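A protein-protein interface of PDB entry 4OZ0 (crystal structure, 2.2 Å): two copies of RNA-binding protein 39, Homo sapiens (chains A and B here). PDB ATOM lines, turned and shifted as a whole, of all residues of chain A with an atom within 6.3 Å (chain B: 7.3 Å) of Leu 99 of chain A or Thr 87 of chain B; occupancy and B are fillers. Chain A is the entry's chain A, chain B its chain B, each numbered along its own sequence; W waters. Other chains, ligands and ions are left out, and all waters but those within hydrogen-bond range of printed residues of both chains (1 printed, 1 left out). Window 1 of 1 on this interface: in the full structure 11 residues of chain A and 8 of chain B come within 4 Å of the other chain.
The side-chain amide nitrogen (ND2) of Asn 98 of chain A is in hydrogen-bond range of the side-chain amide oxygen (OE1) of Gln 56 of chain B (3.4 Å).
The side-chain amide oxygen of Asn 98 of chain A sits close to the backbone carbonyl oxygen of Pro 94 of chain A, at 3.3 Å. The backbone carbonyl oxygen (O) of Met 85 of chain B sits at hydrogen-bond distance from the side-chain amide nitrogen (ND2) of Asn 15 of chain B (3.1 Å). The backbone NH (N) of Gly 78 of chain B is in hydrogen-bond range of the backbone carbonyl oxygen (O) of Ile 86 of chain B (3.0 Å). O of Gln 56 of chain B is in hydrogen-bond range of N of Asn 15 of chain B (2.8 Å). N of Ser 14 of chain B lies within hydrogen-bond range of O of Thr 87 of chain B (2.8 Å). The backbone NH of Asn 15 of chain B sits at hydrogen-bond distance from the backbone carbonyl oxygen of Gly 57 of chain B (3.3 Å).
Among the printed residues, merely in contact across the chains: Tyr 60 of chain A with Gly 78 of chain B, Leu 99 of chain A with His 77 of chain B, Tyr 60 of chain A with Met 85 of chain B, Thr 95 of chain A with Asn 15 of chain B, Tyr 60 of chain A with His 77 of chain B, Leu 99 of chain A with Thr 87 of chain B, Leu 99 of chain A with Met 85 of chain B and Thr 95 of chain A with Met 85 of chain B.
Printed residues of chain B within 4 Å of Leu 99 of chain A: His 77 (3.5 Å), Met 85 (3.8 Å) and Thr 87 (3.8 Å). Of the printed residues of chain A, Thr 87 of chain B touches Leu 99 (3.8 Å). Of the printed residues of chain A, Met 85 of chain B touches Tyr 60, Thr 95 and Leu 99. Of the printed residues of chain B, Thr 95 of chain A touches Asn 15 and Met 85. Printed residues of chain A within 4 Å of His 77 of chain B: Tyr 60 (3.7 Å) and Leu 99 (3.5 Å). The nearest printed residue of chain A that does not touch Thr 87 of chain B is Thr 95 of chain A (5.4 Å).
Of the 9 printed residues of chain A, 4 touch a printed residue of chain B. Hydrophobic or aromatic side chains of chain A within 4 Å of the printed part of chain B: Tyr 60 and Leu 99. Of the 21 printed residues of chain B, 6 touch a printed residue of chain A. Among the printed residues, no Asp or Glu carboxylate lies within 4 Å of a Lys or Arg side-chain nitrogen of the other chain.
No position is printed for both chains.
Water W1 lies within hydrogen-bond range of ND2 of Asn 98 of chain A and OE1 of Gln 56 of chain B.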
ATOM      1  N   TYR A  60      26.407   3.619 -29.395  1.00  0.00           N
ATOM      2  CA  TYR A  60      25.327   4.393 -28.792  1.00  0.00           C
ATOM      3  C   TYR A  60      24.558   5.127 -29.872  1.00  0.00           C
ATOM      4  O   TYR A  60      25.151   5.650 -30.811  1.00  0.00           O
ATOM      5  CB  TYR A  60      25.882   5.374 -27.762  1.00  0.00           C
ATOM      6  CG  TYR A  60      26.542   4.671 -26.603  1.00  0.00           C
ATOM      7  CD1 TYR A  60      25.843   4.410 -25.435  1.00  0.00           C
ATOM      8  CD2 TYR A  60      27.865   4.250 -26.684  1.00  0.00           C
ATOM      9  CE1 TYR A  60      26.443   3.758 -24.378  1.00  0.00           C
ATOM     10  CE2 TYR A  60      28.471   3.596 -25.633  1.00  0.00           C
ATOM     11  CZ  TYR A  60      27.757   3.354 -24.483  1.00  0.00           C
ATOM     12  OH  TYR A  60      28.357   2.703 -23.432  1.00  0.00           O
ATOM     13  N   PRO A  94      18.235  11.170 -19.301  1.00  0.00           N
ATOM     14  CA  PRO A  94      19.223  11.847 -18.450  1.00  0.00           C
ATOM     15  C   PRO A  94      20.584  11.150 -18.446  1.00  0.00           C
ATOM     16  O   PRO A  94      21.609  11.826 -18.491  1.00  0.00           O
ATOM     17  CB  PRO A  94      18.582  11.804 -17.054  1.00  0.00           C
ATOM     18  CG  PRO A  94      17.129  11.583 -17.293  1.00  0.00           C
ATOM     19  CD  PRO A  94      17.026  10.783 -18.552  1.00  0.00           C
ATOM     20  N   THR A  95      20.591   9.822 -18.395  1.00  0.00           N
ATOM     21  CA  THR A  95      21.841   9.066 -18.444  1.00  0.00           C
ATOM     22  C   THR A  95      22.555   9.252 -19.778  1.00  0.00           C
ATOM     23  O   THR A  95      23.758   9.516 -19.825  1.00  0.00           O
ATOM     24  CB  THR A  95      21.592   7.566 -18.210  1.00  0.00           C
ATOM     25  OG1 THR A  95      20.898   7.393 -16.969  1.00  0.00           O
ATOM     26  CG2 THR A  95      22.908   6.793 -18.164  1.00  0.00           C
ATOM     27  N   TYR A  96      21.803   9.117 -20.862  1.00  0.00           N
ATOM     28  CA  TYR A  96      22.356   9.255 -22.204  1.00  0.00           C
ATOM     29  C   TYR A  96      22.824  10.683 -22.429  1.00  0.00           C
ATOM     30  O   TYR A  96      23.857  10.926 -23.053  1.00  0.00           O
ATOM     31  CB  TYR A  96      21.317   8.851 -23.243  1.00  0.00           C
ATOM     32  CG  TYR A  96      21.878   8.614 -24.621  1.00  0.00           C
ATOM     33  CD1 TYR A  96      22.024   9.658 -25.524  1.00  0.00           C
ATOM     34  CD2 TYR A  96      22.279   7.347 -25.014  1.00  0.00           C
ATOM     35  CE1 TYR A  96      22.531   9.443 -26.789  1.00  0.00           C
ATOM     36  CE2 TYR A  96      22.786   7.119 -26.279  1.00  0.00           C
ATOM     37  CZ  TYR A  96      22.915   8.174 -27.163  1.00  0.00           C
ATOM     38  OH  TYR A  96      23.423   7.969 -28.429  1.00  0.00           O
ATOM     39  N   HIS A  97      22.036  11.625 -21.929  1.00  0.00           N
ATOM     40  CA  HIS A  97      22.356  13.036 -22.041  1.00  0.00           C
ATOM     41  C   HIS A  97      23.560  13.373 -21.169  1.00  0.00           C
ATOM     42  O   HIS A  97      24.373  14.218 -21.526  1.00  0.00           O
ATOM     43  CB  HIS A  97      21.142  13.882 -21.668  1.00  0.00           C
ATOM     44  CG  HIS A  97      20.038  13.803 -22.675  1.00  0.00           C
ATOM     45  ND1 HIS A  97      20.244  13.350 -23.963  1.00  0.00           N
ATOM     46  CD2 HIS A  97      18.721  14.107 -22.591  1.00  0.00           C
ATOM     47  CE1 HIS A  97      19.104  13.385 -24.627  1.00  0.00           C
ATOM     48  NE2 HIS A  97      18.163  13.841 -23.818  1.00  0.00           N
ATOM     49  N   ASN A  98      23.675  12.708 -20.024  1.00  0.00           N
ATOM     50  CA  ASN A  98      24.834  12.906 -19.165  1.00  0.00           C
ATOM     51  C   ASN A  98      26.088  12.360 -19.843  1.00  0.00           C
ATOM     52  O   ASN A  98      27.151  12.979 -19.790  1.00  0.00           O
ATOM     53  CB  ASN A  98      24.627  12.228 -17.809  1.00  0.00           C
ATOM     54  CG  ASN A  98      23.868  13.101 -16.822  1.00  0.00           C
ATOM     55  OD1 ASN A  98      23.413  14.198 -17.158  1.00  0.00           O
ATOM     56  ND2 ASN A  98      23.723  12.613 -15.596  1.00  0.00           N
ATOM     57  N   LEU A  99      25.961  11.201 -20.483  1.00  0.00           N
ATOM     58  CA  LEU A  99      27.064  10.626 -21.248  1.00  0.00           C
ATOM     59  C   LEU A  99      27.325  11.417 -22.532  1.00  0.00           C
ATOM     60  O   LEU A  99      28.475  11.623 -22.918  1.00  0.00           O
ATOM     61  CB  LEU A  99      26.780   9.160 -21.580  1.00  0.00           C
ATOM     62  CG  LEU A  99      27.848   8.445 -22.415  1.00  0.00           C
ATOM     63  CD1 LEU A  99      29.220   8.534 -21.754  1.00  0.00           C
ATOM     64  CD2 LEU A  99      27.460   6.992 -22.645  1.00  0.00           C
ATOM     65  N   PHE A 100      26.248  11.850 -23.186  1.00  0.00           N
ATOM     66  CA  PHE A 100      26.338  12.608 -24.436  1.00  0.00           C
ATOM     67  C   PHE A 100      25.513  13.891 -24.335  1.00  0.00           C
ATOM     68  O   PHE A 100      24.384  13.945 -24.823  1.00  0.00           O
ATOM     69  CB  PHE A 100      25.849  11.770 -25.624  1.00  0.00           C
ATOM     70  CG  PHE A 100      26.586  10.472 -25.803  1.00  0.00           C
ATOM     71  CD1 PHE A 100      27.895  10.460 -26.259  1.00  0.00           C
ATOM     72  CD2 PHE A 100      25.968   9.265 -25.522  1.00  0.00           C
ATOM     73  CE1 PHE A 100      28.575   9.268 -26.431  1.00  0.00           C
ATOM     74  CE2 PHE A 100      26.640   8.069 -25.692  1.00  0.00           C
ATOM     75  CZ  PHE A 100      27.948   8.070 -26.146  1.00  0.00           C
ATOM     76  N   PRO A 101      26.073  14.926 -23.686  1.00  0.00           N
ATOM     77  CA  PRO A 101      25.414  16.229 -23.519  1.00  0.00           C
ATOM     78  C   PRO A 101      24.854  16.811 -24.816  1.00  0.00           C
ATOM     79  O   PRO A 101      23.763  17.372 -24.805  1.00  0.00           O
ATOM     80  CB  PRO A 101      26.531  17.119 -22.966  1.00  0.00           C
ATOM     81  CG  PRO A 101      27.461  16.189 -22.277  1.00  0.00           C
ATOM     82  CD  PRO A 101      27.334  14.840 -22.928  1.00  0.00           C
ATOM     83  N   PHE B  11      40.128   6.672 -12.586  1.00  0.00           N
ATOM     84  CA  PHE B  11      38.871   7.000 -13.225  1.00  0.00           C
ATOM     85  C   PHE B  11      37.755   7.170 -12.209  1.00  0.00           C
ATOM     86  O   PHE B  11      37.834   6.703 -11.072  1.00  0.00           O
ATOM     87  CB  PHE B  11      38.506   5.928 -14.256  1.00  0.00           C
ATOM     88  CG  PHE B  11      38.435   4.543 -13.693  1.00  0.00           C
ATOM     89  CD1 PHE B  11      37.234   4.021 -13.243  1.00  0.00           C
ATOM     90  CD2 PHE B  11      39.571   3.756 -13.623  1.00  0.00           C
ATOM     91  CE1 PHE B  11      37.172   2.741 -12.729  1.00  0.00           C
ATOM     92  CE2 PHE B  11      39.515   2.477 -13.111  1.00  0.00           C
ATOM     93  CZ  PHE B  11      38.316   1.968 -12.664  1.00  0.00           C
ATOM     94  N   GLN B  12      36.721   7.872 -12.648  1.00  0.00           N
ATOM     95  CA  GLN B  12      35.546   8.125 -11.847  1.00  0.00           C
ATOM     96  C   GLN B  12      34.403   7.367 -12.480  1.00  0.00           C
ATOM     97  O   GLN B  12      34.058   7.608 -13.636  1.00  0.00           O
ATOM     98  CB  GLN B  12      35.238   9.622 -11.788  1.00  0.00           C
ATOM     99  CG  GLN B  12      33.952   9.984 -11.059  1.00  0.00           C
ATOM    100  CD  GLN B  12      33.361  11.287 -11.554  1.00  0.00           C
ATOM    101  OE1 GLN B  12      33.117  11.453 -12.750  1.00  0.00           O
ATOM    102  NE2 GLN B  12      33.135  12.223 -10.638  1.00  0.00           N
ATOM    103  N   LEU B  13      33.828   6.441 -11.727  1.00  0.00           N
ATOM    104  CA  LEU B  13      32.623   5.769 -12.171  1.00  0.00           C
ATOM    105  C   LEU B  13      31.460   6.663 -11.776  1.00  0.00           C
ATOM    106  O   LEU B  13      31.507   7.307 -10.732  1.00  0.00           O
ATOM    107  CB  LEU B  13      32.507   4.386 -11.537  1.00  0.00           C
ATOM    108  CG  LEU B  13      33.623   3.416 -11.927  1.00  0.00           C
ATOM    109  CD1 LEU B  13      33.606   2.199 -11.021  1.00  0.00           C
ATOM    110  CD2 LEU B  13      33.507   3.004 -13.390  1.00  0.00           C
ATOM    111  N   SER B  14      30.429   6.712 -12.612  1.00  0.00           N
ATOM    112  CA  SER B  14      29.224   7.467 -12.295  1.00  0.00           C
ATOM    113  C   SER B  14      28.026   6.546 -12.348  1.00  0.00           C
ATOM    114  O   SER B  14      28.087   5.471 -12.943  1.00  0.00           O
ATOM    115  CB  SER B  14      29.029   8.633 -13.268  1.00  0.00           C
ATOM    116  OG  SER B  14      30.138   9.513 -13.243  1.00  0.00           O
ATOM    117  N   ASN B  15      26.936   6.980 -11.728  1.00  0.00           N
ATOM    118  CA  ASN B  15      25.683   6.250 -11.773  1.00  0.00           C
ATOM    119  C   ASN B  15      25.816   4.888 -11.101  1.00  0.00           C
ATOM    120  O   ASN B  15      25.034   3.975 -11.369  1.00  0.00           O
ATOM    121  CB  ASN B  15      25.228   6.092 -13.227  1.00  0.00           C
ATOM    122  CG  ASN B  15      23.719   6.181 -13.394  1.00  0.00           C
ATOM    123  OD1 ASN B  15      22.992   6.549 -12.470  1.00  0.00           O
ATOM    124  ND2 ASN B  15      23.244   5.858 -14.591  1.00  0.00           N
ATOM    125  N   MET B  16      26.808   4.761 -10.222  1.00  0.00           N
ATOM    126  CA  MET B  16      26.997   3.540  -9.451  1.00  0.00           C
ATOM    127  C   MET B  16      25.936   3.430  -8.358  1.00  0.00           C
ATOM    128  O   MET B  16      25.664   2.341  -7.856  1.00  0.00           O
ATOM    129  CB  MET B  16      28.391   3.504  -8.818  1.00  0.00           C
ATOM    130  CG  MET B  16      29.551   3.350  -9.799  1.00  0.00           C
ATOM    131  SD  MET B  16      29.712   1.715 -10.538  1.00  0.00           S
ATOM    132  CE  MET B  16      30.086   0.699  -9.118  1.00  0.00           C
ATOM    133  N   GLN B  56      25.605  12.070  -8.046  1.00  0.00           N
ATOM    134  CA  GLN B  56      25.725  11.316  -9.295  1.00  0.00           C
ATOM    135  C   GLN B  56      26.204   9.876  -9.098  1.00  0.00           C
ATOM    136  O   GLN B  56      26.475   9.171 -10.070  1.00  0.00           O
ATOM    137  CB  GLN B  56      26.693  12.038 -10.240  1.00  0.00           C
ATOM    138  CG  GLN B  56      26.133  13.301 -10.884  1.00  0.00           C
ATOM    139  CD  GLN B  56      25.394  13.035 -12.185  1.00  0.00           C
ATOM    140  OE1 GLN B  56      25.669  12.061 -12.889  1.00  0.00           O
ATOM    141  NE2 GLN B  56      24.448  13.909 -12.513  1.00  0.00           N
ATOM    142  N   GLY B  57      26.292   9.437  -7.849  1.00  0.00           N
ATOM    143  CA  GLY B  57      26.718   8.083  -7.549  1.00  0.00           C
ATOM    144  C   GLY B  57      28.141   7.838  -8.007  1.00  0.00           C
ATOM    145  O   GLY B  57      28.425   6.890  -8.741  1.00  0.00           O
ATOM    146  N   ASN B  58      29.047   8.689  -7.552  1.00  0.00           N
ATOM    147  CA  ASN B  58      30.420   8.622  -8.006  1.00  0.00           C
ATOM    148  C   ASN B  58      31.252   7.645  -7.179  1.00  0.00           C
ATOM    149  O   ASN B  58      31.168   7.621  -5.949  1.00  0.00           O
ATOM    150  CB  ASN B  58      31.036  10.020  -7.984  1.00  0.00           C
ATOM    151  CG  ASN B  58      30.379  10.957  -8.990  1.00  0.00           C
ATOM    152  OD1 ASN B  58      30.005  10.543 -10.090  1.00  0.00           O
ATOM    153  ND2 ASN B  58      30.219  12.218  -8.611  1.00  0.00           N
ATOM    154  N   VAL B  59      32.045   6.837  -7.874  1.00  0.00           N
ATOM    155  CA  VAL B  59      33.028   5.975  -7.236  1.00  0.00           C
ATOM    156  C   VAL B  59      34.376   6.252  -7.867  1.00  0.00           C
ATOM    157  O   VAL B  59      34.526   6.202  -9.090  1.00  0.00           O
ATOM    158  CB  VAL B  59      32.692   4.485  -7.381  1.00  0.00           C
ATOM    159  CG1 VAL B  59      33.748   3.633  -6.675  1.00  0.00           C
ATOM    160  CG2 VAL B  59      31.310   4.196  -6.823  1.00  0.00           C
ATOM    161  N   VAL B  73      38.368   0.302 -17.054  1.00  0.00           N
ATOM    162  CA  VAL B  73      37.443   1.252 -17.669  1.00  0.00           C
ATOM    163  C   VAL B  73      36.764   0.668 -18.903  1.00  0.00           C
ATOM    164  O   VAL B  73      35.553   0.810 -19.074  1.00  0.00           O
ATOM    165  CB  VAL B  73      38.164   2.570 -18.046  1.00  0.00           C
ATOM    166  CG1 VAL B  73      37.326   3.424 -19.006  1.00  0.00           C
ATOM    167  CG2 VAL B  73      38.497   3.356 -16.796  1.00  0.00           C
ATOM    168  N   LEU B  76      34.297  -1.542 -17.737  1.00  0.00           N
ATOM    169  CA  LEU B  76      33.297  -0.955 -16.842  1.00  0.00           C
ATOM    170  C   LEU B  76      32.385   0.067 -17.523  1.00  0.00           C
ATOM    171  O   LEU B  76      31.193   0.127 -17.224  1.00  0.00           O
ATOM    172  CB  LEU B  76      33.983  -0.296 -15.641  1.00  0.00           C
ATOM    173  CG  LEU B  76      34.533  -1.224 -14.552  1.00  0.00           C
ATOM    174  CD1 LEU B  76      35.492  -0.480 -13.639  1.00  0.00           C
ATOM    175  CD2 LEU B  76      33.394  -1.814 -13.740  1.00  0.00           C
ATOM    176  N   HIS B  77      32.927   0.875 -18.427  1.00  0.00           N
ATOM    177  CA  HIS B  77      32.127   1.915 -19.069  1.00  0.00           C
ATOM    178  C   HIS B  77      31.105   1.283 -20.004  1.00  0.00           C
ATOM    179  O   HIS B  77      31.447   0.415 -20.805  1.00  0.00           O
ATOM    180  CB  HIS B  77      33.013   2.890 -19.840  1.00  0.00           C
ATOM    181  CG  HIS B  77      32.244   3.914 -20.612  1.00  0.00           C
ATOM    182  ND1 HIS B  77      31.921   3.755 -21.940  1.00  0.00           N
ATOM    183  CD2 HIS B  77      31.729   5.108 -20.237  1.00  0.00           C
ATOM    184  CE1 HIS B  77      31.241   4.812 -22.354  1.00  0.00           C
ATOM    185  NE2 HIS B  77      31.113   5.645 -21.340  1.00  0.00           N
ATOM    186  N   GLY B  78      29.851   1.713 -19.902  1.00  0.00           N
ATOM    187  CA  GLY B  78      28.797   1.129 -20.712  1.00  0.00           C
ATOM    188  C   GLY B  78      28.181  -0.071 -20.020  1.00  0.00           C
ATOM    189  O   GLY B  78      27.081  -0.504 -20.363  1.00  0.00           O
ATOM    190  N   ARG B  79      28.903  -0.616 -19.046  1.00  0.00           N
ATOM    191  CA  ARG B  79      28.443  -1.786 -18.321  1.00  0.00           C
ATOM    192  C   ARG B  79      27.230  -1.361 -17.521  1.00  0.00           C
ATOM    193  O   ARG B  79      27.070  -0.179 -17.222  1.00  0.00           O
ATOM    194  CB  ARG B  79      29.541  -2.330 -17.405  1.00  0.00           C
ATOM    195  CG  ARG B  79      29.331  -3.749 -16.909  1.00  0.00           C
ATOM    196  CD  ARG B  79      30.352  -4.087 -15.833  1.00  0.00           C
ATOM    197  NE  ARG B  79      30.602  -5.524 -15.716  1.00  0.00           N
ATOM    198  CZ  ARG B  79      31.543  -6.187 -16.386  1.00  0.00           C
ATOM    199  NH1 ARG B  79      32.343  -5.557 -17.238  1.00  0.00           N
ATOM    200  NH2 ARG B  79      31.688  -7.493 -16.200  1.00  0.00           N
ATOM    201  N   LYS B  84      21.310   0.490 -13.789  1.00  0.00           N
ATOM    202  CA  LYS B  84      21.756   1.766 -14.335  1.00  0.00           C
ATOM    203  C   LYS B  84      23.024   1.586 -15.157  1.00  0.00           C
ATOM    204  O   LYS B  84      23.872   0.760 -14.819  1.00  0.00           O
ATOM    205  CB  LYS B  84      22.001   2.768 -13.206  1.00  0.00           C
ATOM    206  CG  LYS B  84      20.786   3.012 -12.319  1.00  0.00           C
ATOM    207  CD  LYS B  84      21.147   3.837 -11.090  1.00  0.00           C
ATOM    208  CE  LYS B  84      21.850   3.001 -10.024  1.00  0.00           C
ATOM    209  NZ  LYS B  84      20.906   2.096  -9.304  1.00  0.00           N
ATOM    210  N   MET B  85      23.166   2.355 -16.232  1.00  0.00           N
ATOM    211  CA  MET B  85      24.355   2.219 -17.049  1.00  0.00           C
ATOM    212  C   MET B  85      25.433   3.042 -16.374  1.00  0.00           C
ATOM    213  O   MET B  85      25.326   4.265 -16.274  1.00  0.00           O
ATOM    214  CB  MET B  85      24.124   2.736 -18.471  1.00  0.00           C
ATOM    215  CG  MET B  85      25.275   2.440 -19.422  1.00  0.00           C
ATOM    216  SD  MET B  85      25.002   3.029 -21.106  1.00  0.00           S
ATOM    217  CE  MET B  85      24.867   4.799 -20.833  1.00  0.00           C
ATOM    218  N   ILE B  86      26.476   2.368 -15.909  1.00  0.00           N
ATOM    219  CA  ILE B  86      27.592   3.062 -15.294  1.00  0.00           C
ATOM    220  C   ILE B  86      28.460   3.638 -16.389  1.00  0.00           C
ATOM    221  O   ILE B  86      28.603   3.053 -17.463  1.00  0.00           O
ATOM    222  CB  ILE B  86      28.418   2.163 -14.346  1.00  0.00           C
ATOM    223  CG1 ILE B  86      29.057   0.988 -15.083  1.00  0.00           C
ATOM    224  CG2 ILE B  86      27.534   1.668 -13.217  1.00  0.00           C
ATOM    225  CD1 ILE B  86      30.093   0.254 -14.261  1.00  0.00           C
ATOM    226  N   THR B  87      29.015   4.815 -16.128  1.00  0.00           N
ATOM    227  CA  THR B  87      29.940   5.443 -17.053  1.00  0.00           C
ATOM    228  C   THR B  87      31.238   5.734 -16.330  1.00  0.00           C
ATOM    229  O   THR B  87      31.244   6.216 -15.195  1.00  0.00           O
ATOM    230  CB  THR B  87      29.373   6.742 -17.647  1.00  0.00           C
ATOM    231  OG1 THR B  87      28.809   7.542 -16.603  1.00  0.00           O
ATOM    232  CG2 THR B  87      28.304   6.429 -18.683  1.00  0.00           C
ATOM    233  N   ALA B  88      32.338   5.405 -16.989  1.00  0.00           N
ATOM    234  CA  ALA B  88      33.655   5.676 -16.459  1.00  0.00           C
ATOM    235  C   ALA B  88      34.196   6.873 -17.199  1.00  0.00           C
ATOM    236  O   ALA B  88      34.123   6.955 -18.424  1.00  0.00           O
ATOM    237  CB  ALA B  88      34.570   4.483 -16.612  1.00  0.00           C
ATOM    238  N   ALA B  89      34.737   7.801 -16.430  1.00  0.00           N
ATOM    239  CA  ALA B  89      35.448   8.939 -16.966  1.00  0.00           C
ATOM    240  C   ALA B  89      36.783   8.946 -16.266  1.00  0.00           C
ATOM    241  O   ALA B  89      36.848   8.845 -15.041  1.00  0.00           O
ATOM    242  CB  ALA B  89      34.687  10.232 -16.734  1.00  0.00           C
HETATM  243  O   HOH W   1      24.605   9.778 -14.952  1.00  0.00           O
